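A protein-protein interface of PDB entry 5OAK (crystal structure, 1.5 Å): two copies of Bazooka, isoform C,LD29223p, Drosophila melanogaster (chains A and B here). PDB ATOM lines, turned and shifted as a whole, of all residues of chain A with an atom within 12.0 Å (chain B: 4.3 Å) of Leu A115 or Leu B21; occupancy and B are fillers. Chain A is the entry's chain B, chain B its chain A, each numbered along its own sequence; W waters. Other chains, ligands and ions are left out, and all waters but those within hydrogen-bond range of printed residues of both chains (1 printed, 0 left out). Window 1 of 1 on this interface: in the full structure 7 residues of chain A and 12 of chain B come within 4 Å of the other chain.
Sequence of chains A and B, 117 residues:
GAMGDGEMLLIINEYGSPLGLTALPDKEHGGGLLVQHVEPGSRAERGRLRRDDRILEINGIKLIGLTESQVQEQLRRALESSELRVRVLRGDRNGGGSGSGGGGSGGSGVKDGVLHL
Printed residues of chain B within 4 Å of Leu A115: Leu B21 (3.8 Å), Thr B22 (3.3 Å), Ala B23 (2.7 Å), Leu B33 (3.9 Å), Gln B72 (3.997 Å) and Leu B75 (3.5 Å). Of the printed residues of chain A, Leu B21 touches Leu A115 (3.8 Å), His A116 (3.5 Å) and Leu A117 (2.9 Å). Gly B20 touches just one residue of chain A: Leu A117 (3.0 Å). Ala B23 touches just these residues of chain A: Val A114 and Leu A115. No residue of chain A comes within 4 Å of Val B35. No residue of chain A comes within 4 Å of Leu B49. Of the printed residues of chain B, His A116 touches Leu B21 (3.5 Å) and Thr B22 (3.3 Å). Printed residues of chain B within 4 Å of Val A114: Thr B22 (3.8 Å) and Ala B23 (3.5 Å). Printed residues of chain A within 4 Å of Thr B22: Val A114 (3.8 Å), Leu A115 (3.3 Å) and His A116 (3.3 Å). Printed residues of chain B within 4 Å of Val A110: Gln B72 (3.6 Å). Of the printed residues of chain A, Gln B72 touches Val A110 and Leu A115. Lys A111 touches none of the printed residues of chain B. Ser A108 touches none of the printed residues of chain B. The nearest printed residue of chain B that does not touch His A116 is Ala B23 (5.1 Å).
Along chain B the printed residues that touch a printed residue of chain A span positions 19 to 75. Along chain A the printed residues that touch a printed residue of chain B span positions 110 to 117. Among the printed residues, 15 pairs touch across the chains.
Water W1 lies within hydrogen-bond range of NE2 of Gln B72 (2.8 Å) and O of Gly A113 (2.9 Å).
No position is printed for both chains.
N of Leu B19 is in hydrogen-bond range of O of Leu A117 (2.6 Å). The chain-end carboxylate (OXT) of Leu A117 sits at hydrogen-bond distance from the backbone NH (N) of Gly B20 (3.0 Å). The backbone carbonyl oxygen (O) of Leu B21 lies within hydrogen-bond range of the backbone NH (N) of Leu A117, at 2.9 Å. The side-chain hydroxyl (OG1) of Thr B22 is in hydrogen-bond range of a ring nitrogen (ND1) of His A116 (3.3 Å). O of Ala B23 sits at hydrogen-bond distance from N of Leu A115 (2.7 Å).
The backbone carbonyl oxygen (O) of His B37 lies within hydrogen-bond range of the backbone NH (N) of Thr B22, 2.9 Å away. The backbone carbonyl oxygen (O) of Leu B33 lies within hydrogen-bond range of the backbone NH (N) of Ile B55, at 2.7 Å. The backbone NH (N) of His A116 is in hydrogen-bond range of the backbone carbonyl oxygen (O) of Gly A109 (2.8 Å).
Among the printed residues, merely in contact across the chains: Leu A115 with Thr B22 (3.3 Å), Leu A115 with Leu B75 (3.5 Å), His A116 with Leu B21 (3.5 Å), Val A114 with Ala B23 (3.5 Å), Val A110 with Gln B72 (3.6 Å), Leu A117 with Leu B75 (3.6 Å), Val A114 with Thr B22 (3.8 Å), Leu A115 with Leu B21 (3.8 Å), Leu A115 with Leu B33 (3.9 Å) and Leu A115 with Gln B72 (3.997 Å).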
ATOM      1  N   GLY A 107     -20.724  27.738   9.268  1.00  0.00           N
ATOM      2  CA  GLY A 107     -20.929  26.303   9.272  1.00  0.00           C
ATOM      3  C   GLY A 107     -19.736  25.549   9.829  1.00  0.00           C
ATOM      4  O   GLY A 107     -18.806  26.151  10.375  1.00  0.00           O
ATOM      5  N   SER A 108     -19.774  24.224   9.698  1.00  0.00           N
ATOM      6  CA  SER A 108     -18.688  23.362  10.172  1.00  0.00           C
ATOM      7  C   SER A 108     -18.488  22.086   9.339  1.00  0.00           C
ATOM      8  O   SER A 108     -18.828  20.979   9.779  1.00  0.00           O
ATOM      9  CB  SER A 108     -18.911  22.958  11.632  1.00  0.00           C
ATOM     10  OG  SER A 108     -17.928  22.007  12.036  1.00  0.00           O
ATOM     11  N   GLY A 109     -17.962  22.246   8.135  1.00  0.00           N
ATOM     12  CA  GLY A 109     -17.353  21.136   7.429  1.00  0.00           C
ATOM     13  C   GLY A 109     -15.883  21.166   7.805  1.00  0.00           C
ATOM     14  O   GLY A 109     -15.041  21.435   6.971  1.00  0.00           O
ATOM     15  N   VAL A 110     -15.598  20.904   9.086  1.00  0.00           N
ATOM     16  CA  VAL A 110     -14.242  20.943   9.621  1.00  0.00           C
ATOM     17  C   VAL A 110     -13.879  19.594  10.257  1.00  0.00           C
ATOM     18  O   VAL A 110     -14.496  19.173  11.245  1.00  0.00           O
ATOM     19  CB  VAL A 110     -14.069  22.042  10.700  1.00  0.00           C
ATOM     20  CG1 VAL A 110     -12.603  22.114  11.158  1.00  0.00           C
ATOM     21  CG2 VAL A 110     -14.602  23.396  10.216  1.00  0.00           C
ATOM     22  N   LYS A 111     -12.868  18.932   9.705  1.00  0.00           N
ATOM     23  CA  LYS A 111     -12.507  17.596  10.168  1.00  0.00           C
ATOM     24  C   LYS A 111     -10.998  17.490  10.413  1.00  0.00           C
ATOM     25  O   LYS A 111     -10.227  17.370   9.457  1.00  0.00           O
ATOM     26  CB  LYS A 111     -12.966  16.553   9.142  1.00  0.00           C
ATOM     27  N   ASP A 112     -10.583  17.547  11.682  1.00  0.00           N
ATOM     28  CA  ASP A 112      -9.158  17.564  12.043  1.00  0.00           C
ATOM     29  C   ASP A 112      -8.356  18.626  11.250  1.00  0.00           C
ATOM     30  O   ASP A 112      -7.336  18.333  10.599  1.00  0.00           O
ATOM     31  CB  ASP A 112      -8.546  16.177  11.839  1.00  0.00           C
ATOM     32  N   GLY A 113      -8.832  19.865  11.300  1.00  0.00           N
ATOM     33  CA  GLY A 113      -8.155  20.960  10.624  1.00  0.00           C
ATOM     34  C   GLY A 113      -8.496  21.136   9.164  1.00  0.00           C
ATOM     35  O   GLY A 113      -8.470  22.255   8.695  1.00  0.00           O
ATOM     36  N   VAL A 114      -8.801  20.046   8.466  1.00  0.00           N
ATOM     37  CA  VAL A 114      -9.212  20.107   7.069  1.00  0.00           C
ATOM     38  C   VAL A 114     -10.584  20.744   6.915  1.00  0.00           C
ATOM     39  O   VAL A 114     -11.512  20.398   7.636  1.00  0.00           O
ATOM     40  CB  VAL A 114      -9.242  18.718   6.451  1.00  0.00           C
ATOM     41  CG1 VAL A 114      -9.622  18.794   4.990  1.00  0.00           C
ATOM     42  CG2 VAL A 114      -7.882  18.075   6.622  1.00  0.00           C
ATOM     43  N   LEU A 115     -10.712  21.662   5.954  1.00  0.00           N
ATOM     44  CA  LEU A 115     -11.918  22.452   5.769  1.00  0.00           C
ATOM     45  C   LEU A 115     -12.549  22.100   4.429  1.00  0.00           C
ATOM     46  O   LEU A 115     -11.869  22.108   3.405  1.00  0.00           O
ATOM     47  CB  LEU A 115     -11.566  23.947   5.827  1.00  0.00           C
ATOM     48  CG  LEU A 115     -10.822  24.418   7.091  1.00  0.00           C
ATOM     49  CD1 LEU A 115     -10.414  25.861   6.979  1.00  0.00           C
ATOM     50  CD2 LEU A 115     -11.665  24.222   8.358  1.00  0.00           C
ATOM     51  N   HIS A 116     -13.848  21.803   4.430  1.00  0.00           N
ATOM     52  CA  HIS A 116     -14.594  21.689   3.193  1.00  0.00           C
ATOM     53  C   HIS A 116     -15.506  22.889   3.109  1.00  0.00           C
ATOM     54  O   HIS A 116     -16.255  23.170   4.031  1.00  0.00           O
ATOM     55  CB  HIS A 116     -15.414  20.412   3.141  1.00  0.00           C
ATOM     56  CG  HIS A 116     -14.584  19.184   3.267  1.00  0.00           C
ATOM     57  ND1 HIS A 116     -14.193  18.435   2.180  1.00  0.00           N
ATOM     58  CD2 HIS A 116     -14.010  18.610   4.347  1.00  0.00           C
ATOM     59  CE1 HIS A 116     -13.437  17.430   2.589  1.00  0.00           C
ATOM     60  NE2 HIS A 116     -13.318  17.510   3.901  1.00  0.00           N
ATOM     61  N   LEU A 117     -15.416  23.597   2.009  1.00  0.00           N
ATOM     62  CA  LEU A 117     -16.176  24.822   1.793  1.00  0.00           C
ATOM     63  C   LEU A 117     -16.915  24.785   0.475  1.00  0.00           C
ATOM     64  O   LEU A 117     -17.830  25.578   0.283  1.00  0.00           O
ATOM     65  CB  LEU A 117     -15.251  26.050   1.756  1.00  0.00           C
ATOM     66  CG  LEU A 117     -14.543  26.590   2.959  1.00  0.00           C
ATOM     67  CD1 LEU A 117     -13.302  25.793   3.049  1.00  0.00           C
ATOM     68  CD2 LEU A 117     -14.289  28.060   2.687  1.00  0.00           C
ATOM     69  OXT LEU A 117     -16.566  24.010  -0.439  1.00  0.00           O
ATOM     70  N   LEU B  19     -18.952  25.446  -2.100  1.00  0.00           N
ATOM     71  CA  LEU B  19     -18.275  26.103  -3.216  1.00  0.00           C
ATOM     72  C   LEU B  19     -17.332  25.186  -3.960  1.00  0.00           C
ATOM     73  O   LEU B  19     -16.915  25.484  -5.090  1.00  0.00           O
ATOM     74  CB  LEU B  19     -17.539  27.349  -2.713  1.00  0.00           C
ATOM     75  CG  LEU B  19     -18.520  28.304  -2.035  1.00  0.00           C
ATOM     76  CD1 LEU B  19     -17.820  29.544  -1.581  1.00  0.00           C
ATOM     77  CD2 LEU B  19     -19.714  28.693  -2.969  1.00  0.00           C
ATOM     78  N   GLY B  20     -17.020  24.054  -3.359  1.00  0.00           N
ATOM     79  CA  GLY B  20     -16.226  23.049  -4.056  1.00  0.00           C
ATOM     80  C   GLY B  20     -14.745  23.036  -3.733  1.00  0.00           C
ATOM     81  O   GLY B  20     -13.946  22.603  -4.539  1.00  0.00           O
ATOM     82  N   LEU B  21     -14.364  23.473  -2.540  1.00  0.00           N
ATOM     83  CA  LEU B  21     -12.971  23.668  -2.065  1.00  0.00           C
ATOM     84  C   LEU B  21     -12.680  22.719  -0.903  1.00  0.00           C
ATOM     85  O   LEU B  21     -13.469  22.765   0.067  1.00  0.00           O
ATOM     86  CB  LEU B  21     -12.771  25.138  -1.552  1.00  0.00           C
ATOM     87  CG  LEU B  21     -11.393  25.584  -1.119  1.00  0.00           C
ATOM     88  CD1 LEU B  21     -10.551  25.434  -2.333  1.00  0.00           C
ATOM     89  CD2 LEU B  21     -11.405  27.021  -0.646  1.00  0.00           C
ATOM     90  N   THR B  22     -11.565  22.010  -0.908  1.00  0.00           N
ATOM     91  CA  THR B  22     -11.053  21.383   0.284  1.00  0.00           C
ATOM     92  C   THR B  22      -9.715  22.061   0.586  1.00  0.00           C
ATOM     93  O   THR B  22      -8.900  22.166  -0.304  1.00  0.00           O
ATOM     94  CB  THR B  22     -10.829  19.889   0.059  1.00  0.00           C
ATOM     95  OG1 THR B  22     -12.077  19.283  -0.270  1.00  0.00           O
ATOM     96  CG2 THR B  22     -10.274  19.221   1.313  1.00  0.00           C
ATOM     97  N   ALA B  23      -9.512  22.523   1.820  1.00  0.00           N
ATOM     98  CA  ALA B  23      -8.295  23.239   2.168  1.00  0.00           C
ATOM     99  C   ALA B  23      -7.854  22.799   3.540  1.00  0.00           C
ATOM    100  O   ALA B  23      -8.615  22.308   4.366  1.00  0.00           O
ATOM    101  CB  ALA B  23      -8.533  24.714   2.161  1.00  0.00           C
ATOM    102  N   LEU B  33      -4.097  29.027   3.909  1.00  0.00           N
ATOM    103  CA  LEU B  33      -4.777  27.767   3.656  1.00  0.00           C
ATOM    104  C   LEU B  33      -4.234  27.193   2.370  1.00  0.00           C
ATOM    105  O   LEU B  33      -4.184  27.888   1.349  1.00  0.00           O
ATOM    106  CB  LEU B  33      -6.293  27.980   3.530  1.00  0.00           C
ATOM    107  CG  LEU B  33      -6.999  28.407   4.856  1.00  0.00           C
ATOM    108  CD1 LEU B  33      -8.454  28.935   4.525  1.00  0.00           C
ATOM    109  CD2 LEU B  33      -7.007  27.279   5.881  1.00  0.00           C
ATOM    110  N   VAL B  35      -4.826  24.778  -0.755  1.00  0.00           N
ATOM    111  CA  VAL B  35      -5.940  24.116  -1.440  1.00  0.00           C
ATOM    112  C   VAL B  35      -5.554  22.676  -1.800  1.00  0.00           C
ATOM    113  O   VAL B  35      -4.557  22.451  -2.494  1.00  0.00           O
ATOM    114  CB  VAL B  35      -6.335  24.931  -2.695  1.00  0.00           C
ATOM    115  CG1 VAL B  35      -7.472  24.194  -3.496  1.00  0.00           C
ATOM    116  CG2 VAL B  35      -6.794  26.344  -2.266  1.00  0.00           C
ATOM    117  N   HIS B  37      -8.037  20.303  -2.987  1.00  0.00           N
ATOM    118  CA  HIS B  37      -8.877  19.796  -4.052  1.00  0.00           C
ATOM    119  C   HIS B  37      -9.892  20.835  -4.427  1.00  0.00           C
ATOM    120  O   HIS B  37     -10.345  21.590  -3.555  1.00  0.00           O
ATOM    121  CB  HIS B  37      -9.589  18.526  -3.619  1.00  0.00           C
ATOM    122  CG  HIS B  37     -10.253  17.824  -4.741  1.00  0.00           C
ATOM    123  ND1 HIS B  37     -11.627  17.795  -4.895  1.00  0.00           N
ATOM    124  CD2 HIS B  37      -9.737  17.173  -5.811  1.00  0.00           C
ATOM    125  CE1 HIS B  37     -11.933  17.108  -5.983  1.00  0.00           C
ATOM    126  NE2 HIS B  37     -10.809  16.724  -6.558  1.00  0.00           N
ATOM    127  N   LEU B  49      -9.600  28.827  -8.752  1.00  0.00           N
ATOM    128  CA  LEU B  49      -8.861  28.175  -7.673  1.00  0.00           C
ATOM    129  C   LEU B  49      -8.311  26.838  -8.178  1.00  0.00           C
ATOM    130  O   LEU B  49      -8.996  26.103  -8.922  1.00  0.00           O
ATOM    131  CB  LEU B  49      -9.773  27.929  -6.465  1.00  0.00           C
ATOM    132  CG  LEU B  49      -9.891  29.040  -5.448  1.00  0.00           C
ATOM    133  CD1 LEU B  49     -10.865  28.580  -4.399  1.00  0.00           C
ATOM    134  CD2 LEU B  49      -8.581  29.375  -4.723  1.00  0.00           C
ATOM    135  N   ILE B  55      -3.907  30.150  -0.054  1.00  0.00           N
ATOM    136  CA  ILE B  55      -4.823  31.278   0.131  1.00  0.00           C
ATOM    137  C   ILE B  55      -4.262  32.147   1.252  1.00  0.00           C
ATOM    138  O   ILE B  55      -4.076  31.662   2.371  1.00  0.00           O
ATOM    139  CB  ILE B  55      -6.225  30.800   0.510  1.00  0.00           C
ATOM    140  CG1 ILE B  55      -6.835  30.007  -0.661  1.00  0.00           C
ATOM    141  CG2 ILE B  55      -7.079  32.013   0.887  1.00  0.00           C
ATOM    142  CD1 ILE B  55      -8.106  29.212  -0.195  1.00  0.00           C
ATOM    143  N   GLN B  72     -10.912  30.061  10.860  1.00  0.00           N
ATOM    144  CA  GLN B  72     -12.196  29.394  10.667  1.00  0.00           C
ATOM    145  C   GLN B  72     -13.315  30.424  10.841  1.00  0.00           C
ATOM    146  O   GLN B  72     -14.286  30.442  10.089  1.00  0.00           O
ATOM    147  CB  GLN B  72     -12.364  28.235  11.648  1.00  0.00           C
ATOM    148  CG  GLN B  72     -11.574  27.021  11.210  1.00  0.00           C
ATOM    149  CD  GLN B  72     -11.593  25.942  12.265  1.00  0.00           C
ATOM    150  OE1 GLN B  72     -12.410  25.993  13.174  1.00  0.00           O
ATOM    151  NE2 GLN B  72     -10.678  24.983  12.171  1.00  0.00           N
ATOM    152  N   LEU B  75     -13.554  32.634   7.834  1.00  0.00           N
ATOM    153  CA  LEU B  75     -14.237  31.934   6.743  1.00  0.00           C
ATOM    154  C   LEU B  75     -15.746  31.971   6.940  1.00  0.00           C
ATOM    155  O   LEU B  75     -16.495  32.176   5.992  1.00  0.00           O
ATOM    156  CB  LEU B  75     -13.835  30.481   6.670  1.00  0.00           C
ATOM    157  CG  LEU B  75     -12.465  30.328   6.095  1.00  0.00           C
ATOM    158  CD1 LEU B  75     -11.947  28.902   6.369  1.00  0.00           C
ATOM    159  CD2 LEU B  75     -12.530  30.584   4.617  1.00  0.00           C
HETATM  160  O   HOH W   1      -8.545  24.549  10.473  1.00  0.00           O
